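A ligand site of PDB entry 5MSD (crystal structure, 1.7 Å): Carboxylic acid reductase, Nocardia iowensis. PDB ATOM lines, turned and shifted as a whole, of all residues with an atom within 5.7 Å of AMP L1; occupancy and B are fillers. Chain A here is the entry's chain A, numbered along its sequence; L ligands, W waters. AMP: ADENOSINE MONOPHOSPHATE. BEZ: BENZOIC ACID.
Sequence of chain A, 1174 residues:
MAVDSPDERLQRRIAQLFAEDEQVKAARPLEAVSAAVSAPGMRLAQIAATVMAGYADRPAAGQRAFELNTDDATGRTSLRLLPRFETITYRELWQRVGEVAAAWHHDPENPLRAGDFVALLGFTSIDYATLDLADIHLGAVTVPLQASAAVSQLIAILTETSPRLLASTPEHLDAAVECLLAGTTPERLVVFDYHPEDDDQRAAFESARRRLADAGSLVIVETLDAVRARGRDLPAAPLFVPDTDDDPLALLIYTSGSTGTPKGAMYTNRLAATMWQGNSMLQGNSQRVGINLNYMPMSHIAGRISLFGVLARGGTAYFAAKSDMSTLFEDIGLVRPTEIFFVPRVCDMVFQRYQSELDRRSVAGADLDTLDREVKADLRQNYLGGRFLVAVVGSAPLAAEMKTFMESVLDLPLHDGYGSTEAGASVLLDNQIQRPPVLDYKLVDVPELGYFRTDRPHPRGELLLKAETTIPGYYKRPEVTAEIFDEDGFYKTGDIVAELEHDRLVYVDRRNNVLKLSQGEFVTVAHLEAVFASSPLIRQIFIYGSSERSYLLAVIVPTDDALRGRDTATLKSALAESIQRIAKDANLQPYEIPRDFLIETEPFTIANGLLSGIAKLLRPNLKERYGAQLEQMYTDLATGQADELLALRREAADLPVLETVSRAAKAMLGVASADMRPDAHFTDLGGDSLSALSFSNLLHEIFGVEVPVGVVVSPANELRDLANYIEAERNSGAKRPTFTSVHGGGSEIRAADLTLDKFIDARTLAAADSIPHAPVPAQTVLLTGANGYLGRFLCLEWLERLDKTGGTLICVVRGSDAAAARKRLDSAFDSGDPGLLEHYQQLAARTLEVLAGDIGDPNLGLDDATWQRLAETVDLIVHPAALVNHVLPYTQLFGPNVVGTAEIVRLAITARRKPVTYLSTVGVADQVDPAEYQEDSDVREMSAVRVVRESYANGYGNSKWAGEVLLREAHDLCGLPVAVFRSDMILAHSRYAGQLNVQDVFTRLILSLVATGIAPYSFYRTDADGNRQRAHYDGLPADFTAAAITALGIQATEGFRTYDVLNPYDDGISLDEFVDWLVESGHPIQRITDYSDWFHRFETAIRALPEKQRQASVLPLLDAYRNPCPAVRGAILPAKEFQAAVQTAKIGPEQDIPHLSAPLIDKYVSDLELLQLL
OH of Tyr 507 lies within hydrogen-bond range of O2' of AMP L1 (2.8 Å).
The backbone carbonyl oxygen (O) of Gly 417 is in hydrogen-bond range of a nitrogen (N6) of AMP L1, 2.8 Å away.
NH1 of Arg 510 is in hydrogen-bond range of O3' of AMP L1.
A ring nitrogen (NE2) of His 300 is in hydrogen-bond range of an oxygen (O2P) of AMP L1 (3.0 Å).
The backbone NH of Ser 395 sits at hydrogen-bond distance from a nitrogen (N7) of AMP L1 (3.2 Å).
The side-chain amino group (NZ) of Lys 616 lies within hydrogen-bond range of an oxygen (O4') of AMP L1, 2.9 Å away.
OG1 of Thr 421 lies within hydrogen-bond range of O1P of AMP L1 (2.9 Å).
An oxygen (O3') of AMP L1 lies within hydrogen-bond range of the side-chain carboxylate of Asp 495, 2.7 Å away.
A nitrogen (N6) of AMP L1 sits at hydrogen-bond distance from the side-chain carboxylate of Asp 416, 2.7 Å away.
O1P of AMP L1 lies within hydrogen-bond range of N of Thr 421, 3.0 Å away.
An oxygen (O1) of BEZ L2 sits close to an oxygen (O2P) of AMP L1 (2.5 Å).
OG of Ser 420 lies close to N of Glu 422, 3.4 Å away.
NZ of Lys 616 is in hydrogen-bond range of O of Ser 395 (2.8 Å).
OD2 of Asp 495 sits at hydrogen-bond distance from OH of Tyr 418 (2.5 Å).
O of Val 393 is in hydrogen-bond range of N of Gly 417 (2.8 Å).
The guanidinium group (NH1) of Arg 510 is in hydrogen-bond range of the backbone carbonyl oxygen (O) of Thr 493, 2.8 Å away.
The side-chain hydroxyl (OG1) of Thr 493 is in hydrogen-bond range of the backbone NH (N) of Asp 495, 3.1 Å away.
N of Arg 510 is in hydrogen-bond range of OH of Tyr 507.
OD1 of Asp 495 lies within salt-bridge range of NH1 of Arg 510 (2.7 Å).
N1 of AMP L1 sits close to O of Ala 396 (3.5 Å).
Merely in contact with AMP L1: Thr 255 (3.6 Å), Gly 394 (3.9 Å), Pro 397 (3.3 Å), Tyr 418 (3.6 Å), Gly 419 (3.3 Å), Ser 420 (3.8 Å) and Glu 422 (3.96 Å).
Hydrophobic or aromatic side chains within 4 Å of AMP L1: His 300, Pro 397, Tyr 418 and Tyr 507.
The nearest printed residue that does not touch AMP L1 is Val 393 (4.3 Å).
Water W4 lies within hydrogen-bond range of O2P of AMP L1 (2.8 Å), O of Ser 395 (2.9 Å), NZ of Lys 616 (3.0 Å) and O2 of BEZ L2 (3.0 Å).
Water W2 lies within hydrogen-bond range of a nitrogen (N1) of AMP L1 and the side-chain carboxylate (OD2) of Asp 416.
Water W1 bridges an oxygen (O3') of AMP L1 (3.2 Å) and the guanidinium group of Arg 510 (3.4 Å).
Water W3 bridges O of Thr 493 (2.7 Å) and O3' of AMP L1 (3.4 Å).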
ATOM      1  N   THR A 255      24.839  10.117  -7.502  1.00  0.00           N
ATOM      2  CA  THR A 255      23.778   9.655  -6.619  1.00  0.00           C
ATOM      3  C   THR A 255      24.375   8.531  -5.776  1.00  0.00           C
ATOM      4  O   THR A 255      25.219   7.761  -6.266  1.00  0.00           O
ATOM      5  CB  THR A 255      22.520   9.189  -7.441  1.00  0.00           C
ATOM      6  OG1 THR A 255      21.451   8.790  -6.567  1.00  0.00           O
ATOM      7  CG2 THR A 255      22.875   8.034  -8.371  1.00  0.00           C
ATOM      8  N   GLY A 257      22.499   6.482  -3.074  1.00  0.00           N
ATOM      9  CA  GLY A 257      21.644   5.434  -2.524  1.00  0.00           C
ATOM     10  C   GLY A 257      21.831   5.355  -1.017  1.00  0.00           C
ATOM     11  O   GLY A 257      21.980   6.380  -0.361  1.00  0.00           O
ATOM     12  N   HIS A 300      20.797  17.730  -8.283  1.00  0.00           N
ATOM     13  CA  HIS A 300      19.717  16.727  -8.200  1.00  0.00           C
ATOM     14  C   HIS A 300      18.784  16.844  -9.386  1.00  0.00           C
ATOM     15  O   HIS A 300      18.535  17.958  -9.846  1.00  0.00           O
ATOM     16  CB  HIS A 300      18.893  16.868  -6.908  1.00  0.00           C
ATOM     17  CG  HIS A 300      18.063  15.654  -6.603  1.00  0.00           C
ATOM     18  ND1 HIS A 300      16.823  15.429  -7.155  1.00  0.00           N
ATOM     19  CD2 HIS A 300      18.330  14.559  -5.841  1.00  0.00           C
ATOM     20  CE1 HIS A 300      16.347  14.275  -6.731  1.00  0.00           C
ATOM     21  NE2 HIS A 300      17.248  13.721  -5.944  1.00  0.00           N
ATOM     22  N   ILE A 301      18.233  15.731  -9.860  1.00  0.00           N
ATOM     23  CA  ILE A 301      17.351  15.824 -11.016  1.00  0.00           C
ATOM     24  C   ILE A 301      16.114  16.695 -10.759  1.00  0.00           C
ATOM     25  O   ILE A 301      15.642  17.366 -11.659  1.00  0.00           O
ATOM     26  CB  ILE A 301      16.881  14.436 -11.518  1.00  0.00           C
ATOM     27  CG1 ILE A 301      16.234  13.645 -10.392  1.00  0.00           C
ATOM     28  CG2 ILE A 301      18.032  13.671 -12.082  1.00  0.00           C
ATOM     29  CD1 ILE A 301      15.309  12.575 -10.937  1.00  0.00           C
ATOM     30  N   VAL A 393       4.349  16.415  -4.539  1.00  0.00           N
ATOM     31  CA  VAL A 393       5.305  16.019  -3.528  1.00  0.00           C
ATOM     32  C   VAL A 393       6.025  14.766  -4.039  1.00  0.00           C
ATOM     33  O   VAL A 393       5.428  13.918  -4.714  1.00  0.00           O
ATOM     34  CB  VAL A 393       4.630  15.789  -2.136  1.00  0.00           C
ATOM     35  CG1 VAL A 393       3.642  14.613  -2.170  1.00  0.00           C
ATOM     36  CG2 VAL A 393       5.664  15.579  -1.039  1.00  0.00           C
ATOM     37  N   GLY A 394       7.321  14.676  -3.753  1.00  0.00           N
ATOM     38  CA  GLY A 394       8.133  13.564  -4.210  1.00  0.00           C
ATOM     39  C   GLY A 394       9.450  13.505  -3.462  1.00  0.00           C
ATOM     40  O   GLY A 394       9.653  14.268  -2.502  1.00  0.00           O
ATOM     41  N   SER A 395      10.298  12.555  -3.888  1.00  0.00           N
ATOM     42  CA  SER A 395      11.659  12.278  -3.402  1.00  0.00           C
ATOM     43  C   SER A 395      11.695  11.358  -2.180  1.00  0.00           C
ATOM     44  O   SER A 395      12.698  10.695  -1.928  1.00  0.00           O
ATOM     45  CB  SER A 395      12.436  13.585  -3.105  1.00  0.00           C
ATOM     46  OG  SER A 395      12.224  14.030  -1.771  1.00  0.00           O
ATOM     47  N   ALA A 396      10.591  11.289  -1.447  1.00  0.00           N
ATOM     48  CA  ALA A 396      10.509  10.532  -0.198  1.00  0.00           C
ATOM     49  C   ALA A 396       9.042  10.345   0.176  1.00  0.00           C
ATOM     50  O   ALA A 396       8.181  11.056  -0.351  1.00  0.00           O
ATOM     51  CB  ALA A 396      11.281  11.250   0.936  1.00  0.00           C
ATOM     52  N   PRO A 397       8.736   9.380   1.058  1.00  0.00           N
ATOM     53  CA  PRO A 397       7.314   9.178   1.364  1.00  0.00           C
ATOM     54  C   PRO A 397       6.699  10.284   2.213  1.00  0.00           C
ATOM     55  O   PRO A 397       7.347  10.862   3.106  1.00  0.00           O
ATOM     56  CB  PRO A 397       7.314   7.852   2.127  1.00  0.00           C
ATOM     57  CG  PRO A 397       8.662   7.739   2.709  1.00  0.00           C
ATOM     58  CD  PRO A 397       9.588   8.364   1.685  1.00  0.00           C
ATOM     59  N   LEU A 398       5.439  10.589   1.930  1.00  0.00           N
ATOM     60  CA  LEU A 398       4.665  11.492   2.758  1.00  0.00           C
ATOM     61  C   LEU A 398       3.544  10.671   3.401  1.00  0.00           C
ATOM     62  O   LEU A 398       2.845   9.960   2.700  1.00  0.00           O
ATOM     63  CB  LEU A 398       4.098  12.649   1.940  1.00  0.00           C
ATOM     64  CG  LEU A 398       3.463  13.807   2.710  1.00  0.00           C
ATOM     65  CD1 LEU A 398       4.540  14.596   3.441  1.00  0.00           C
ATOM     66  CD2 LEU A 398       2.661  14.699   1.765  1.00  0.00           C
ATOM     67  N   ASP A 416       1.256  12.894  -5.568  1.00  0.00           N
ATOM     68  CA  ASP A 416       2.399  12.115  -5.130  1.00  0.00           C
ATOM     69  C   ASP A 416       3.134  11.597  -6.358  1.00  0.00           C
ATOM     70  O   ASP A 416       2.628  10.758  -7.105  1.00  0.00           O
ATOM     71  CB  ASP A 416       1.958  10.970  -4.225  1.00  0.00           C
ATOM     72  CG  ASP A 416       3.101  10.041  -3.841  1.00  0.00           C
ATOM     73  OD1 ASP A 416       4.274  10.499  -3.798  1.00  0.00           O
ATOM     74  OD2 ASP A 416       2.831   8.857  -3.574  1.00  0.00           O
ATOM     75  N   GLY A 417       4.331  12.128  -6.566  1.00  0.00           N
ATOM     76  CA  GLY A 417       5.157  11.767  -7.716  1.00  0.00           C
ATOM     77  C   GLY A 417       6.326  10.905  -7.295  1.00  0.00           C
ATOM     78  O   GLY A 417       7.177  11.343  -6.527  1.00  0.00           O
ATOM     79  N   TYR A 418       6.360   9.679  -7.783  1.00  0.00           N
ATOM     80  CA  TYR A 418       7.467   8.770  -7.541  1.00  0.00           C
ATOM     81  C   TYR A 418       8.357   8.685  -8.783  1.00  0.00           C
ATOM     82  O   TYR A 418       7.889   8.497  -9.894  1.00  0.00           O
ATOM     83  CB  TYR A 418       6.964   7.373  -7.165  1.00  0.00           C
ATOM     84  CG  TYR A 418       8.022   6.298  -7.299  1.00  0.00           C
ATOM     85  CD1 TYR A 418       8.177   5.601  -8.497  1.00  0.00           C
ATOM     86  CD2 TYR A 418       8.867   5.993  -6.242  1.00  0.00           C
ATOM     87  CE1 TYR A 418       9.164   4.623  -8.643  1.00  0.00           C
ATOM     88  CE2 TYR A 418       9.847   5.005  -6.369  1.00  0.00           C
ATOM     89  CZ  TYR A 418       9.989   4.333  -7.572  1.00  0.00           C
ATOM     90  OH  TYR A 418      10.952   3.358  -7.709  1.00  0.00           O
ATOM     91  N   GLY A 419       9.665   8.835  -8.580  1.00  0.00           N
ATOM     92  CA  GLY A 419      10.626   8.611  -9.636  1.00  0.00           C
ATOM     93  C   GLY A 419      12.007   8.473  -9.036  1.00  0.00           C
ATOM     94  O   GLY A 419      12.153   8.403  -7.807  1.00  0.00           O
ATOM     95  N   SER A 420      13.030   8.452  -9.883  1.00  0.00           N
ATOM     96  CA  SER A 420      14.381   8.322  -9.385  1.00  0.00           C
ATOM     97  C   SER A 420      15.360   8.874 -10.394  1.00  0.00           C
ATOM     98  O   SER A 420      15.010   9.092 -11.559  1.00  0.00           O
ATOM     99  CB  SER A 420      14.702   6.859  -9.065  1.00  0.00           C
ATOM    100  OG  SER A 420      14.803   6.079 -10.248  1.00  0.00           O
ATOM    101  N   THR A 421      16.582   9.104  -9.938  1.00  0.00           N
ATOM    102  CA  THR A 421      17.657   9.514 -10.830  1.00  0.00           C
ATOM    103  C   THR A 421      17.832   8.479 -11.935  1.00  0.00           C
ATOM    104  O   THR A 421      18.009   8.840 -13.122  1.00  0.00           O
ATOM    105  CB  THR A 421      18.959   9.704 -10.061  1.00  0.00           C
ATOM    106  OG1 THR A 421      18.759  10.697  -9.037  1.00  0.00           O
ATOM    107  CG2 THR A 421      20.084  10.162 -11.010  1.00  0.00           C
ATOM    108  N   GLU A 422      17.729   7.206 -11.582  1.00  0.00           N
ATOM    109  CA  GLU A 422      17.953   6.132 -12.564  1.00  0.00           C
ATOM    110  C   GLU A 422      16.788   5.925 -13.521  1.00  0.00           C
ATOM    111  O   GLU A 422      16.999   5.618 -14.694  1.00  0.00           O
ATOM    112  CB  GLU A 422      18.266   4.816 -11.870  1.00  0.00           C
ATOM    113  CG  GLU A 422      19.630   4.804 -11.230  1.00  0.00           C
ATOM    114  CD  GLU A 422      19.625   5.362  -9.819  1.00  0.00           C
ATOM    115  OE1 GLU A 422      18.585   5.944  -9.408  1.00  0.00           O
ATOM    116  OE2 GLU A 422      20.649   5.195  -9.132  1.00  0.00           O
ATOM    117  N   THR A 493      14.518  -1.296  -9.222  1.00  0.00           N
ATOM    118  CA  THR A 493      14.403  -0.019  -8.516  1.00  0.00           C
ATOM    119  C   THR A 493      14.931  -0.062  -7.081  1.00  0.00           C
ATOM    120  O   THR A 493      15.230   0.977  -6.506  1.00  0.00           O
ATOM    121  CB  THR A 493      12.955   0.449  -8.447  1.00  0.00           C
ATOM    122  OG1 THR A 493      12.150  -0.551  -7.798  1.00  0.00           O
ATOM    123  CG2 THR A 493      12.412   0.700  -9.842  1.00  0.00           C
ATOM    124  N   ASP A 495      12.919  -0.745  -4.842  1.00  0.00           N
ATOM    125  CA  ASP A 495      11.748  -0.266  -4.120  1.00  0.00           C
ATOM    126  C   ASP A 495      10.661  -1.335  -4.062  1.00  0.00           C
ATOM    127  O   ASP A 495      10.388  -1.981  -5.054  1.00  0.00           O
ATOM    128  CB  ASP A 495      11.181   0.994  -4.783  1.00  0.00           C
ATOM    129  CG  ASP A 495      12.146   2.181  -4.690  1.00  0.00           C
ATOM    130  OD1 ASP A 495      12.907   2.216  -3.718  1.00  0.00           O
ATOM    131  OD2 ASP A 495      12.153   3.044  -5.590  1.00  0.00           O
ATOM    132  N   TYR A 507       3.599   2.699  -3.367  1.00  0.00           N
ATOM    133  CA  TYR A 507       4.954   2.613  -2.838  1.00  0.00           C
ATOM    134  C   TYR A 507       4.946   2.195  -1.368  1.00  0.00           C
ATOM    135  O   TYR A 507       4.148   2.699  -0.579  1.00  0.00           O
ATOM    136  CB  TYR A 507       5.669   3.951  -2.987  1.00  0.00           C
ATOM    137  CG  TYR A 507       7.086   3.987  -2.462  1.00  0.00           C
ATOM    138  CD1 TYR A 507       8.166   3.678  -3.294  1.00  0.00           C
ATOM    139  CD2 TYR A 507       7.350   4.342  -1.152  1.00  0.00           C
ATOM    140  CE1 TYR A 507       9.484   3.735  -2.808  1.00  0.00           C
ATOM    141  CE2 TYR A 507       8.644   4.396  -0.669  1.00  0.00           C
ATOM    142  CZ  TYR A 507       9.695   4.085  -1.497  1.00  0.00           C
ATOM    143  OH  TYR A 507      10.975   4.150  -0.986  1.00  0.00           O
ATOM    144  N   ASP A 509       8.393   0.922   0.629  1.00  0.00           N
ATOM    145  CA  ASP A 509       9.655   1.477   1.115  1.00  0.00           C
ATOM    146  C   ASP A 509      10.781   0.926   0.272  1.00  0.00           C
ATOM    147  O   ASP A 509      10.547   0.083  -0.610  1.00  0.00           O
ATOM    148  CB  ASP A 509       9.895   1.135   2.601  1.00  0.00           C
ATOM    149  CG  ASP A 509      10.662   2.227   3.358  1.00  0.00           C
ATOM    150  OD1 ASP A 509      11.548   2.916   2.772  1.00  0.00           O
ATOM    151  OD2 ASP A 509      10.373   2.409   4.561  1.00  0.00           O
ATOM    152  N   ARG A 510      11.991   1.415   0.524  1.00  0.00           N
ATOM    153  CA  ARG A 510      13.176   0.831  -0.081  1.00  0.00           C
ATOM    154  C   ARG A 510      13.311  -0.577   0.460  1.00  0.00           C
ATOM    155  O   ARG A 510      13.107  -0.788   1.659  1.00  0.00           O
ATOM    156  CB  ARG A 510      14.444   1.615   0.281  1.00  0.00           C
ATOM    157  CG  ARG A 510      14.457   3.073  -0.121  1.00  0.00           C
ATOM    158  CD  ARG A 510      14.847   3.235  -1.564  1.00  0.00           C
ATOM    159  NE  ARG A 510      16.103   2.583  -1.915  1.00  0.00           N
ATOM    160  CZ  ARG A 510      16.410   2.176  -3.145  1.00  0.00           C
ATOM    161  NH1 ARG A 510      15.541   2.345  -4.139  1.00  0.00           N
ATOM    162  NH2 ARG A 510      17.568   1.589  -3.383  1.00  0.00           N
ATOM    163  N   ILE A 614      18.499  17.701  -0.850  1.00  0.00           N
ATOM    164  CA  ILE A 614      17.066  17.932  -1.004  1.00  0.00           C
ATOM    165  C   ILE A 614      16.306  17.553   0.278  1.00  0.00           C
ATOM    166  O   ILE A 614      15.118  17.241   0.255  1.00  0.00           O
ATOM    167  CB  ILE A 614      16.488  17.173  -2.209  1.00  0.00           C
ATOM    168  CG1 ILE A 614      16.683  15.665  -2.061  1.00  0.00           C
ATOM    169  CG2 ILE A 614      17.138  17.674  -3.512  1.00  0.00           C
ATOM    170  CD1 ILE A 614      15.808  14.871  -2.984  1.00  0.00           C
ATOM    171  N   LYS A 616      16.562  15.108   2.455  1.00  0.00           N
ATOM    172  CA  LYS A 616      16.224  13.723   2.749  1.00  0.00           C
ATOM    173  C   LYS A 616      17.180  13.202   3.817  1.00  0.00           C
ATOM    174  O   LYS A 616      18.357  13.543   3.789  1.00  0.00           O
ATOM    175  CB  LYS A 616      16.329  12.900   1.467  1.00  0.00           C
ATOM    176  CG  LYS A 616      15.832  11.517   1.573  1.00  0.00           C
ATOM    177  CD  LYS A 616      15.703  10.959   0.170  1.00  0.00           C
ATOM    178  CE  LYS A 616      15.063   9.606   0.174  1.00  0.00           C
ATOM    179  NZ  LYS A 616      14.898   9.154  -1.239  1.00  0.00           N
HETATM  180  P   AMP L   1      17.195   9.634  -5.769  1.00  0.00           P
HETATM  181  O1P AMP L   1      17.457   8.953  -7.087  1.00  0.00           O
HETATM  182  O2P AMP L   1      16.389  10.887  -5.891  1.00  0.00           O
HETATM  183  O3P AMP L   1      18.408   9.845  -4.900  1.00  0.00           O
HETATM  184  O5' AMP L   1      16.236   8.695  -4.890  1.00  0.00           O
HETATM  185  C5' AMP L   1      15.169   7.979  -5.473  1.00  0.00           C
HETATM  186  C4' AMP L   1      14.398   7.213  -4.413  1.00  0.00           C
HETATM  187  O4' AMP L   1      13.593   8.141  -3.662  1.00  0.00           O
HETATM  188  C3' AMP L   1      13.402   6.192  -4.927  1.00  0.00           C
HETATM  189  O3' AMP L   1      14.014   4.971  -5.300  1.00  0.00           O
HETATM  190  C2' AMP L   1      12.411   6.066  -3.777  1.00  0.00           C
HETATM  191  O2' AMP L   1      12.896   5.183  -2.774  1.00  0.00           O
HETATM  192  C1' AMP L   1      12.413   7.502  -3.203  1.00  0.00           C
HETATM  193  N9  AMP L   1      11.249   8.246  -3.695  1.00  0.00           N
HETATM  194  C8  AMP L   1      11.190   9.038  -4.767  1.00  0.00           C
HETATM  195  N7  AMP L   1       9.926   9.515  -4.936  1.00  0.00           N
HETATM  196  C5  AMP L   1       9.173   9.020  -3.940  1.00  0.00           C
HETATM  197  C6  AMP L   1       7.763   9.113  -3.519  1.00  0.00           C
HETATM  198  N6  AMP L   1       6.856   9.861  -4.190  1.00  0.00           N
HETATM  199  N1  AMP L   1       7.385   8.408  -2.434  1.00  0.00           N
HETATM  200  C2  AMP L   1       8.259   7.660  -1.737  1.00  0.00           C
HETATM  201  N3  AMP L   1       9.549   7.513  -2.062  1.00  0.00           N
HETATM  202  C4  AMP L   1      10.048   8.170  -3.133  1.00  0.00           C
HETATM  203  C   BEZ L   2      13.564  11.565  -7.048  1.00  0.00           C
HETATM  204  O1  BEZ L   2      14.675  11.431  -7.622  1.00  0.00           O
HETATM  205  O2  BEZ L   2      13.480  11.266  -5.853  1.00  0.00           O
HETATM  206  C1  BEZ L   2      12.369  12.092  -7.779  1.00  0.00           C
HETATM  207  C2  BEZ L   2      12.532  12.790  -8.969  1.00  0.00           C
HETATM  208  C3  BEZ L   2      11.412  13.280  -9.632  1.00  0.00           C
HETATM  209  C4  BEZ L   2      10.130  13.082  -9.114  1.00  0.00           C
HETATM  210  C5  BEZ L   2       9.966  12.384  -7.924  1.00  0.00           C
HETATM  211  C6  BEZ L   2      11.088  11.898  -7.248  1.00  0.00           C
HETATM  212  O   HOH W   1      17.121   4.786  -5.918  1.00  0.00           O
HETATM  213  O   HOH W   2       4.751   7.755  -1.837  1.00  0.00           O
HETATM  214  O   HOH W   3      15.492   3.290  -7.842  1.00  0.00           O
HETATM  215  O   HOH W   4      15.183  11.121  -3.420  1.00  0.00           O
